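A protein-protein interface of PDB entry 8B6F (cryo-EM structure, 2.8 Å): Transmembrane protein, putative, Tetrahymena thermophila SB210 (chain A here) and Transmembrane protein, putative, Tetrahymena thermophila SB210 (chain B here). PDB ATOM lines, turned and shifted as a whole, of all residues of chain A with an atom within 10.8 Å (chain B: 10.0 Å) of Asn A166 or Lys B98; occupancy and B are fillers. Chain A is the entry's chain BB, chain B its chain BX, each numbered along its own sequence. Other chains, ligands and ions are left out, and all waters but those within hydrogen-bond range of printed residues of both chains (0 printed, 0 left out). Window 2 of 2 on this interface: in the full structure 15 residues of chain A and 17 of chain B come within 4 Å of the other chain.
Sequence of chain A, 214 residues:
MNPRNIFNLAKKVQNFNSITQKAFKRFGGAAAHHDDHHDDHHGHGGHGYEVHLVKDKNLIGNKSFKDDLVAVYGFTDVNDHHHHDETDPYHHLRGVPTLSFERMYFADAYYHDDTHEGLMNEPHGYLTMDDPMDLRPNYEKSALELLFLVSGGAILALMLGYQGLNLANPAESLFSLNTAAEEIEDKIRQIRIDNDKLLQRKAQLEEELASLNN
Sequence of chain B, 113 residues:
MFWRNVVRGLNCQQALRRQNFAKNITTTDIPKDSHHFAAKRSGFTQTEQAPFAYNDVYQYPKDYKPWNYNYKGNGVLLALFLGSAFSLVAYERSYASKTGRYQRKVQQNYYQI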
ATOM      1  N   ALA A 157      -0.097   5.918  15.306  1.00  0.00           N
ATOM      2  CA  ALA A 157       0.605   6.944  16.062  1.00  0.00           C
ATOM      3  C   ALA A 157      -0.182   8.236  16.226  1.00  0.00           C
ATOM      4  O   ALA A 157       0.278   9.124  16.952  1.00  0.00           O
ATOM      5  CB  ALA A 157       1.944   7.263  15.388  1.00  0.00           C
ATOM      6  N   LEU A 158      -1.341   8.374  15.583  1.00  0.00           N
ATOM      7  CA  LEU A 158      -2.089   9.623  15.667  1.00  0.00           C
ATOM      8  C   LEU A 158      -3.541   9.403  16.063  1.00  0.00           C
ATOM      9  O   LEU A 158      -4.158  10.277  16.679  1.00  0.00           O
ATOM     10  CB  LEU A 158      -2.030  10.362  14.329  1.00  0.00           C
ATOM     11  CG  LEU A 158      -0.651  10.859  13.891  1.00  0.00           C
ATOM     12  CD1 LEU A 158      -0.706  11.377  12.468  1.00  0.00           C
ATOM     13  CD2 LEU A 158      -0.148  11.937  14.832  1.00  0.00           C
ATOM     14  N   MET A 159      -4.099   8.245  15.720  1.00  0.00           N
ATOM     15  CA  MET A 159      -5.532   8.010  15.839  1.00  0.00           C
ATOM     16  C   MET A 159      -5.895   6.948  16.861  1.00  0.00           C
ATOM     17  O   MET A 159      -6.849   7.134  17.618  1.00  0.00           O
ATOM     18  CB  MET A 159      -6.098   7.609  14.473  1.00  0.00           C
ATOM     19  CG  MET A 159      -5.836   8.642  13.390  1.00  0.00           C
ATOM     20  SD  MET A 159      -6.223   8.047  11.739  1.00  0.00           S
ATOM     21  CE  MET A 159      -5.670   9.434  10.759  1.00  0.00           C
ATOM     22  N   LEU A 160      -5.168   5.836  16.902  1.00  0.00           N
ATOM     23  CA  LEU A 160      -5.504   4.758  17.822  1.00  0.00           C
ATOM     24  C   LEU A 160      -5.419   5.245  19.262  1.00  0.00           C
ATOM     25  O   LEU A 160      -4.368   5.718  19.706  1.00  0.00           O
ATOM     26  CB  LEU A 160      -4.570   3.569  17.597  1.00  0.00           C
ATOM     27  CG  LEU A 160      -4.802   2.333  18.472  1.00  0.00           C
ATOM     28  CD1 LEU A 160      -6.188   1.759  18.256  1.00  0.00           C
ATOM     29  CD2 LEU A 160      -3.746   1.277  18.201  1.00  0.00           C
ATOM     30  N   GLY A 161      -6.525   5.127  19.991  1.00  0.00           N
ATOM     31  CA  GLY A 161      -6.580   5.573  21.367  1.00  0.00           C
ATOM     32  C   GLY A 161      -6.839   7.056  21.538  1.00  0.00           C
ATOM     33  O   GLY A 161      -7.659   7.451  22.372  1.00  0.00           O
ATOM     34  N   TYR A 162      -6.152   7.890  20.758  1.00  0.00           N
ATOM     35  CA  TYR A 162      -6.336   9.332  20.880  1.00  0.00           C
ATOM     36  C   TYR A 162      -7.766   9.741  20.540  1.00  0.00           C
ATOM     37  O   TYR A 162      -8.363  10.572  21.233  1.00  0.00           O
ATOM     38  CB  TYR A 162      -5.337  10.062  19.982  1.00  0.00           C
ATOM     39  CG  TYR A 162      -5.329  11.558  20.177  1.00  0.00           C
ATOM     40  CD1 TYR A 162      -6.217  12.376  19.490  1.00  0.00           C
ATOM     41  CD2 TYR A 162      -4.430  12.154  21.048  1.00  0.00           C
ATOM     42  CE1 TYR A 162      -6.210  13.743  19.669  1.00  0.00           C
ATOM     43  CE2 TYR A 162      -4.415  13.520  21.235  1.00  0.00           C
ATOM     44  CZ  TYR A 162      -5.308  14.310  20.542  1.00  0.00           C
ATOM     45  OH  TYR A 162      -5.295  15.673  20.724  1.00  0.00           O
ATOM     46  N   GLN A 163      -8.331   9.168  19.476  1.00  0.00           N
ATOM     47  CA  GLN A 163      -9.709   9.480  19.103  1.00  0.00           C
ATOM     48  C   GLN A 163     -10.665   9.246  20.264  1.00  0.00           C
ATOM     49  O   GLN A 163     -11.467  10.120  20.611  1.00  0.00           O
ATOM     50  CB  GLN A 163     -10.128   8.634  17.901  1.00  0.00           C
ATOM     51  CG  GLN A 163      -9.671   9.177  16.570  1.00  0.00           C
ATOM     52  CD  GLN A 163     -10.152   8.336  15.409  1.00  0.00           C
ATOM     53  OE1 GLN A 163     -10.872   7.357  15.596  1.00  0.00           O
ATOM     54  NE2 GLN A 163      -9.762   8.718  14.198  1.00  0.00           N
ATOM     55  N   GLY A 164     -10.592   8.067  20.879  1.00  0.00           N
ATOM     56  CA  GLY A 164     -11.505   7.757  21.966  1.00  0.00           C
ATOM     57  C   GLY A 164     -11.284   8.626  23.187  1.00  0.00           C
ATOM     58  O   GLY A 164     -12.242   9.077  23.821  1.00  0.00           O
ATOM     59  N   LEU A 165     -10.024   8.874  23.539  1.00  0.00           N
ATOM     60  CA  LEU A 165      -9.732   9.582  24.779  1.00  0.00           C
ATOM     61  C   LEU A 165     -10.063  11.066  24.672  1.00  0.00           C
ATOM     62  O   LEU A 165     -10.691  11.636  25.570  1.00  0.00           O
ATOM     63  CB  LEU A 165      -8.263   9.390  25.149  1.00  0.00           C
ATOM     64  CG  LEU A 165      -7.817  10.085  26.433  1.00  0.00           C
ATOM     65  CD1 LEU A 165      -8.565   9.544  27.639  1.00  0.00           C
ATOM     66  CD2 LEU A 165      -6.326   9.932  26.608  1.00  0.00           C
ATOM     67  N   ASN A 166      -9.655  11.709  23.578  1.00  0.00           N
ATOM     68  CA  ASN A 166      -9.702  13.165  23.482  1.00  0.00           C
ATOM     69  C   ASN A 166     -10.918  13.657  22.704  1.00  0.00           C
ATOM     70  O   ASN A 166     -11.697  14.466  23.217  1.00  0.00           O
ATOM     71  CB  ASN A 166      -8.407  13.681  22.840  1.00  0.00           C
ATOM     72  CG  ASN A 166      -7.194  13.456  23.721  1.00  0.00           C
ATOM     73  OD1 ASN A 166      -6.852  14.296  24.553  1.00  0.00           O
ATOM     74  ND2 ASN A 166      -6.536  12.314  23.545  1.00  0.00           N
ATOM     75  N   LEU A 167     -11.093  13.191  21.472  1.00  0.00           N
ATOM     76  CA  LEU A 167     -12.229  13.605  20.651  1.00  0.00           C
ATOM     77  C   LEU A 167     -13.424  12.737  21.016  1.00  0.00           C
ATOM     78  O   LEU A 167     -13.671  11.688  20.419  1.00  0.00           O
ATOM     79  CB  LEU A 167     -11.892  13.507  19.168  1.00  0.00           C
ATOM     80  CG  LEU A 167     -11.267  14.768  18.565  1.00  0.00           C
ATOM     81  CD1 LEU A 167     -10.031  15.194  19.334  1.00  0.00           C
ATOM     82  CD2 LEU A 167     -10.932  14.544  17.102  1.00  0.00           C
ATOM     83  N   ALA A 168     -14.174  13.184  22.018  1.00  0.00           N
ATOM     84  CA  ALA A 168     -15.367  12.501  22.487  1.00  0.00           C
ATOM     85  C   ALA A 168     -16.580  13.391  22.261  1.00  0.00           C
ATOM     86  O   ALA A 168     -16.466  14.613  22.143  1.00  0.00           O
ATOM     87  CB  ALA A 168     -15.254  12.133  23.973  1.00  0.00           C
ATOM     88  N   ASN A 169     -17.745  12.764  22.203  1.00  0.00           N
ATOM     89  CA  ASN A 169     -18.970  13.489  21.912  1.00  0.00           C
ATOM     90  C   ASN A 169     -19.216  14.533  22.997  1.00  0.00           C
ATOM     91  O   ASN A 169     -19.319  14.171  24.178  1.00  0.00           O
ATOM     92  CB  ASN A 169     -20.146  12.520  21.831  1.00  0.00           C
ATOM     93  CG  ASN A 169     -21.418  13.184  21.349  1.00  0.00           C
ATOM     94  OD1 ASN A 169     -21.388  14.290  20.813  1.00  0.00           O
ATOM     95  ND2 ASN A 169     -22.544  12.509  21.536  1.00  0.00           N
ATOM     96  N   PRO A 170     -19.317  15.819  22.657  1.00  0.00           N
ATOM     97  CA  PRO A 170     -19.603  16.816  23.699  1.00  0.00           C
ATOM     98  C   PRO A 170     -20.899  16.550  24.441  1.00  0.00           C
ATOM     99  O   PRO A 170     -20.988  16.846  25.638  1.00  0.00           O
ATOM    100  CB  PRO A 170     -19.655  18.134  22.917  1.00  0.00           C
ATOM    101  CG  PRO A 170     -18.844  17.888  21.704  1.00  0.00           C
ATOM    102  CD  PRO A 170     -19.064  16.451  21.352  1.00  0.00           C
ATOM    103  N   ALA A 171     -21.909  16.002  23.765  1.00  0.00           N
ATOM    104  CA  ALA A 171     -23.171  15.706  24.434  1.00  0.00           C
ATOM    105  C   ALA A 171     -22.979  14.660  25.524  1.00  0.00           C
ATOM    106  O   ALA A 171     -23.483  14.813  26.640  1.00  0.00           O
ATOM    107  CB  ALA A 171     -24.206  15.235  23.414  1.00  0.00           C
ATOM    108  N   GLU A 172     -22.250  13.584  25.219  1.00  0.00           N
ATOM    109  CA  GLU A 172     -22.038  12.549  26.225  1.00  0.00           C
ATOM    110  C   GLU A 172     -21.144  13.060  27.347  1.00  0.00           C
ATOM    111  O   GLU A 172     -21.348  12.714  28.516  1.00  0.00           O
ATOM    112  CB  GLU A 172     -21.447  11.293  25.582  1.00  0.00           C
ATOM    113  CG  GLU A 172     -19.931  11.271  25.492  1.00  0.00           C
ATOM    114  CD  GLU A 172     -19.420  10.089  24.697  1.00  0.00           C
ATOM    115  OE1 GLU A 172     -20.249   9.257  24.275  1.00  0.00           O
ATOM    116  OE2 GLU A 172     -18.192   9.992  24.491  1.00  0.00           O
ATOM    117  N   SER A 173     -20.145  13.878  27.014  1.00  0.00           N
ATOM    118  CA  SER A 173     -19.321  14.487  28.051  1.00  0.00           C
ATOM    119  C   SER A 173     -20.169  15.357  28.965  1.00  0.00           C
ATOM    120  O   SER A 173     -20.032  15.306  30.191  1.00  0.00           O
ATOM    121  CB  SER A 173     -18.199  15.314  27.423  1.00  0.00           C
ATOM    122  OG  SER A 173     -17.344  14.503  26.636  1.00  0.00           O
ATOM    123  N   LEU A 177     -20.744  14.802  33.004  1.00  0.00           N
ATOM    124  CA  LEU A 177     -20.416  15.857  33.958  1.00  0.00           C
ATOM    125  C   LEU A 177     -21.644  16.283  34.752  1.00  0.00           C
ATOM    126  O   LEU A 177     -21.546  16.562  35.951  1.00  0.00           O
ATOM    127  CB  LEU A 177     -19.797  17.050  33.231  1.00  0.00           C
ATOM    128  CG  LEU A 177     -18.450  16.796  32.545  1.00  0.00           C
ATOM    129  CD1 LEU A 177     -17.897  18.086  31.966  1.00  0.00           C
ATOM    130  CD2 LEU A 177     -17.435  16.150  33.484  1.00  0.00           C
ATOM    131  N   ALA B  90       2.013   6.190  24.213  1.00  0.00           N
ATOM    132  CA  ALA B  90       1.432   7.500  23.947  1.00  0.00           C
ATOM    133  C   ALA B  90       0.025   7.599  24.517  1.00  0.00           C
ATOM    134  O   ALA B  90      -0.353   8.636  25.074  1.00  0.00           O
ATOM    135  CB  ALA B  90       1.424   7.776  22.443  1.00  0.00           C
ATOM    136  N   TYR B  91      -0.769   6.535  24.387  1.00  0.00           N
ATOM    137  CA  TYR B  91      -2.099   6.549  24.983  1.00  0.00           C
ATOM    138  C   TYR B  91      -2.022   6.614  26.501  1.00  0.00           C
ATOM    139  O   TYR B  91      -2.820   7.312  27.136  1.00  0.00           O
ATOM    140  CB  TYR B  91      -2.902   5.325  24.556  1.00  0.00           C
ATOM    141  CG  TYR B  91      -4.265   5.304  25.204  1.00  0.00           C
ATOM    142  CD1 TYR B  91      -5.302   6.074  24.699  1.00  0.00           C
ATOM    143  CD2 TYR B  91      -4.504   4.544  26.339  1.00  0.00           C
ATOM    144  CE1 TYR B  91      -6.544   6.076  25.296  1.00  0.00           C
ATOM    145  CE2 TYR B  91      -5.745   4.540  26.945  1.00  0.00           C
ATOM    146  CZ  TYR B  91      -6.760   5.308  26.417  1.00  0.00           C
ATOM    147  OH  TYR B  91      -7.999   5.312  27.010  1.00  0.00           O
ATOM    148  N   GLU B  92      -1.073   5.895  27.105  1.00  0.00           N
ATOM    149  CA  GLU B  92      -0.898   5.983  28.550  1.00  0.00           C
ATOM    150  C   GLU B  92      -0.633   7.422  28.971  1.00  0.00           C
ATOM    151  O   GLU B  92      -1.262   7.936  29.903  1.00  0.00           O
ATOM    152  CB  GLU B  92       0.248   5.076  28.993  1.00  0.00           C
ATOM    153  CG  GLU B  92      -0.018   3.594  28.808  1.00  0.00           C
ATOM    154  CD  GLU B  92      -1.035   3.057  29.792  1.00  0.00           C
ATOM    155  OE1 GLU B  92      -1.540   3.844  30.619  1.00  0.00           O
ATOM    156  OE2 GLU B  92      -1.329   1.846  29.739  1.00  0.00           O
ATOM    157  N   ARG B  93       0.307   8.084  28.299  1.00  0.00           N
ATOM    158  CA  ARG B  93       0.631   9.463  28.644  1.00  0.00           C
ATOM    159  C   ARG B  93      -0.561  10.380  28.404  1.00  0.00           C
ATOM    160  O   ARG B  93      -0.822  11.294  29.194  1.00  0.00           O
ATOM    161  CB  ARG B  93       1.844   9.931  27.844  1.00  0.00           C
ATOM    162  CG  ARG B  93       2.536  11.152  28.426  1.00  0.00           C
ATOM    163  CD  ARG B  93       3.268  10.814  29.712  1.00  0.00           C
ATOM    164  NE  ARG B  93       4.060  11.937  30.198  1.00  0.00           N
ATOM    165  CZ  ARG B  93       3.604  12.898  30.991  1.00  0.00           C
ATOM    166  NH1 ARG B  93       2.349  12.912  31.411  1.00  0.00           N
ATOM    167  NH2 ARG B  93       4.429  13.867  31.375  1.00  0.00           N
ATOM    168  N   SER B  94      -1.295  10.152  27.314  1.00  0.00           N
ATOM    169  CA  SER B  94      -2.461  10.978  27.020  1.00  0.00           C
ATOM    170  C   SER B  94      -3.529  10.831  28.094  1.00  0.00           C
ATOM    171  O   SER B  94      -4.134  11.822  28.518  1.00  0.00           O
ATOM    172  CB  SER B  94      -3.034  10.613  25.650  1.00  0.00           C
ATOM    173  OG  SER B  94      -2.100  10.873  24.618  1.00  0.00           O
ATOM    174  N   TYR B  95      -3.780   9.601  28.547  1.00  0.00           N
ATOM    175  CA  TYR B  95      -4.761   9.397  29.607  1.00  0.00           C
ATOM    176  C   TYR B  95      -4.323  10.073  30.897  1.00  0.00           C
ATOM    177  O   TYR B  95      -5.141  10.682  31.595  1.00  0.00           O
ATOM    178  CB  TYR B  95      -4.989   7.905  29.838  1.00  0.00           C
ATOM    179  CG  TYR B  95      -5.908   7.622  31.001  1.00  0.00           C
ATOM    180  CD1 TYR B  95      -7.283   7.750  30.870  1.00  0.00           C
ATOM    181  CD2 TYR B  95      -5.400   7.228  32.231  1.00  0.00           C
ATOM    182  CE1 TYR B  95      -8.126   7.495  31.932  1.00  0.00           C
ATOM    183  CE2 TYR B  95      -6.233   6.971  33.298  1.00  0.00           C
ATOM    184  CZ  TYR B  95      -7.596   7.105  33.142  1.00  0.00           C
ATOM    185  OH  TYR B  95      -8.433   6.849  34.201  1.00  0.00           O
ATOM    186  N   ALA B  96      -3.037   9.983  31.233  1.00  0.00           N
ATOM    187  CA  ALA B  96      -2.548  10.672  32.420  1.00  0.00           C
ATOM    188  C   ALA B  96      -2.767  12.174  32.300  1.00  0.00           C
ATOM    189  O   ALA B  96      -3.190  12.826  33.261  1.00  0.00           O
ATOM    190  CB  ALA B  96      -1.070  10.355  32.636  1.00  0.00           C
ATOM    191  N   SER B  97      -2.474  12.743  31.130  1.00  0.00           N
ATOM    192  CA  SER B  97      -2.669  14.176  30.934  1.00  0.00           C
ATOM    193  C   SER B  97      -4.140  14.557  31.047  1.00  0.00           C
ATOM    194  O   SER B  97      -4.477  15.586  31.643  1.00  0.00           O
ATOM    195  CB  SER B  97      -2.112  14.597  29.576  1.00  0.00           C
ATOM    196  OG  SER B  97      -0.718  14.362  29.508  1.00  0.00           O
ATOM    197  N   LYS B  98      -5.031  13.746  30.472  1.00  0.00           N
ATOM    198  CA  LYS B  98      -6.458  14.037  30.563  1.00  0.00           C
ATOM    199  C   LYS B  98      -6.939  13.997  32.006  1.00  0.00           C
ATOM    200  O   LYS B  98      -7.746  14.835  32.423  1.00  0.00           O
ATOM    201  CB  LYS B  98      -7.252  13.049  29.709  1.00  0.00           C
ATOM    202  CG  LYS B  98      -7.525  13.535  28.298  1.00  0.00           C
ATOM    203  CD  LYS B  98      -8.567  14.640  28.282  1.00  0.00           C
ATOM    204  CE  LYS B  98      -8.784  15.162  26.875  1.00  0.00           C
ATOM    205  NZ  LYS B  98      -9.823  16.227  26.832  1.00  0.00           N
ATOM    206  N   THR B  99      -6.459  13.028  32.783  1.00  0.00           N
ATOM    207  CA  THR B  99      -6.793  12.945  34.198  1.00  0.00           C
ATOM    208  C   THR B  99      -6.039  13.962  35.042  1.00  0.00           C
ATOM    209  O   THR B  99      -6.305  14.063  36.244  1.00  0.00           O
ATOM    210  CB  THR B  99      -6.509  11.539  34.731  1.00  0.00           C
ATOM    211  OG1 THR B  99      -5.126  11.221  34.543  1.00  0.00           O
ATOM    212  CG2 THR B  99      -7.363  10.511  34.010  1.00  0.00           C
ATOM    213  N   GLY B 100      -5.115  14.711  34.451  1.00  0.00           N
ATOM    214  CA  GLY B 100      -4.368  15.711  35.191  1.00  0.00           C
ATOM    215  C   GLY B 100      -3.400  15.118  36.192  1.00  0.00           C
ATOM    216  O   GLY B 100      -3.281  15.630  37.310  1.00  0.00           O
ATOM    217  N   ARG B 101      -2.704  14.050  35.813  1.00  0.00           N
ATOM    218  CA  ARG B 101      -1.720  13.404  36.663  1.00  0.00           C
ATOM    219  C   ARG B 101      -0.465  13.125  35.852  1.00  0.00           C
ATOM    220  O   ARG B 101      -0.522  12.962  34.631  1.00  0.00           O
ATOM    221  CB  ARG B 101      -2.254  12.092  37.246  1.00  0.00           C
ATOM    222  CG  ARG B 101      -3.573  12.225  37.983  1.00  0.00           C
ATOM    223  CD  ARG B 101      -4.103  10.859  38.384  1.00  0.00           C
ATOM    224  NE  ARG B 101      -5.355  10.949  39.124  1.00  0.00           N
ATOM    225  CZ  ARG B 101      -5.446  11.098  40.438  1.00  0.00           C
ATOM    226  NH1 ARG B 101      -4.369  11.193  41.201  1.00  0.00           N
ATOM    227  NH2 ARG B 101      -6.648  11.152  41.003  1.00  0.00           N
ATOM    228  N   TYR B 102       0.675  13.073  36.541  1.00  0.00           N
ATOM    229  CA  TYR B 102       1.922  12.722  35.872  1.00  0.00           C
ATOM    230  C   TYR B 102       1.946  11.267  35.429  1.00  0.00           C
ATOM    231  O   TYR B 102       2.751  10.908  34.565  1.00  0.00           O
ATOM    232  CB  TYR B 102       3.113  12.998  36.790  1.00  0.00           C
ATOM    233  CG  TYR B 102       3.366  14.465  37.040  1.00  0.00           C
ATOM    234  CD1 TYR B 102       3.916  15.272  36.052  1.00  0.00           C
ATOM    235  CD2 TYR B 102       3.069  15.041  38.267  1.00  0.00           C
ATOM    236  CE1 TYR B 102       4.153  16.614  36.276  1.00  0.00           C
ATOM    237  CE2 TYR B 102       3.303  16.381  38.501  1.00  0.00           C
ATOM    238  CZ  TYR B 102       3.845  17.162  37.503  1.00  0.00           C
ATOM    239  OH  TYR B 102       4.080  18.497  37.730  1.00  0.00           O
ATOM    240  N   GLN B 103       1.091  10.423  36.002  1.00  0.00           N
ATOM    241  CA  GLN B 103       1.043   9.018  35.633  1.00  0.00           C
ATOM    242  C   GLN B 103      -0.330   8.467  35.988  1.00  0.00           C
ATOM    243  O   GLN B 103      -1.052   9.033  36.812  1.00  0.00           O
ATOM    244  CB  GLN B 103       2.151   8.221  36.333  1.00  0.00           C
ATOM    245  CG  GLN B 103       2.251   6.772  35.880  1.00  0.00           C
ATOM    246  CD  GLN B 103       3.468   6.068  36.443  1.00  0.00           C
ATOM    247  OE1 GLN B 103       4.272   6.667  37.156  1.00  0.00           O
ATOM    248  NE2 GLN B 103       3.608   4.786  36.123  1.00  0.00           N
ATOM    249  N   ARG B 104      -0.681   7.354  35.347  1.00  0.00           N
ATOM    250  CA  ARG B 104      -1.953   6.701  35.625  1.00  0.00           C
ATOM    251  C   ARG B 104      -2.034   6.292  37.090  1.00  0.00           C
ATOM    252  O   ARG B 104      -1.059   5.817  37.677  1.00  0.00           O
ATOM    253  CB  ARG B 104      -2.119   5.471  34.731  1.00  0.00           C
ATOM    254  CG  ARG B 104      -3.332   4.610  35.065  1.00  0.00           C
ATOM    255  CD  ARG B 104      -3.357   3.341  34.236  1.00  0.00           C
ATOM    256  NE  ARG B 104      -3.584   3.615  32.822  1.00  0.00           N
ATOM    257  CZ  ARG B 104      -4.780   3.737  32.262  1.00  0.00           C
ATOM    258  NH1 ARG B 104      -5.891   3.624  32.971  1.00  0.00           N
ATOM    259  NH2 ARG B 104      -4.864   3.976  30.957  1.00  0.00           N
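CE1 of Tyr B91 touches O of Gly A161, at 3.4 Å. Leu A165 touches Tyr B91. Ser B94 touches Leu A165 (C to CD2, 3.3 Å). Leu A165 touches Tyr B95. CG of Leu A165 touches CG of Lys B98 (3.9 Å). Asn A166 touches Lys B98.
Of chain B, only Lys B98 (3.1 Å) comes within 4 Å of Asn A166. Lys B98 touches two residues of chain A. Tyr A162 touches none of the printed residues of chain B. No residue of chain B comes within 4 Å of Gly A164. Printed residues of chain B within 4 Å of Leu A165: Tyr B91 (3.7 Å), Ser B94 (3.3 Å), Tyr B95 (3.2 Å) and Lys B98 (3.9 Å). No residue of chain B comes within 4 Å of Leu A167. No residue of chain B comes within 4 Å of Ala A168. Ser B94 touches just one residue of chain A: Leu A165. No residue of chain A comes within 4 Å of Ser B97. No residue of chain A comes within 4 Å of Gly B100. Printed residues of chain A within 4 Å of Tyr B95: Leu A165. Printed residues of chain A within 4 Å of Tyr B91: Gly A161 (3.4 Å) and Leu A165 (3.7 Å). Ser A173 touches none of the printed residues of chain B. The nearest residue of chain B that does not touch Asn A166 is Ser B94 (4.4 Å). The nearest printed residue of chain A that does not touch Tyr B95 is Asn A166 (6.3 Å).
The side-chain amide nitrogen of Asn A166 lies close to the backbone carbonyl oxygen of Tyr A162, 3.4 Å away. The backbone carbonyl oxygen (O) of Ala B90 sits at hydrogen-bond distance from the side-chain hydroxyl (OG) of Ser B94 (2.9 Å). OG1 of Thr B99 is in hydrogen-bond range of O of Tyr B95 (3.0 Å).
Of the 18 printed residues of chain A, 3 touch a printed residue of chain B. Hydrophobic or aromatic side chains of chain A that line the printed part of chain B: Leu A165. Printed residues of chain B that touch a printed residue of chain A: Tyr B91, Ser B94, Tyr B95 and Lys B98. Hydrophobic or aromatic side chains of chain B that line the printed part of chain A: Tyr B91 and Tyr B95. Along chain B the printed residues that touch a printed residue of chain A span positions 91 to 98.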
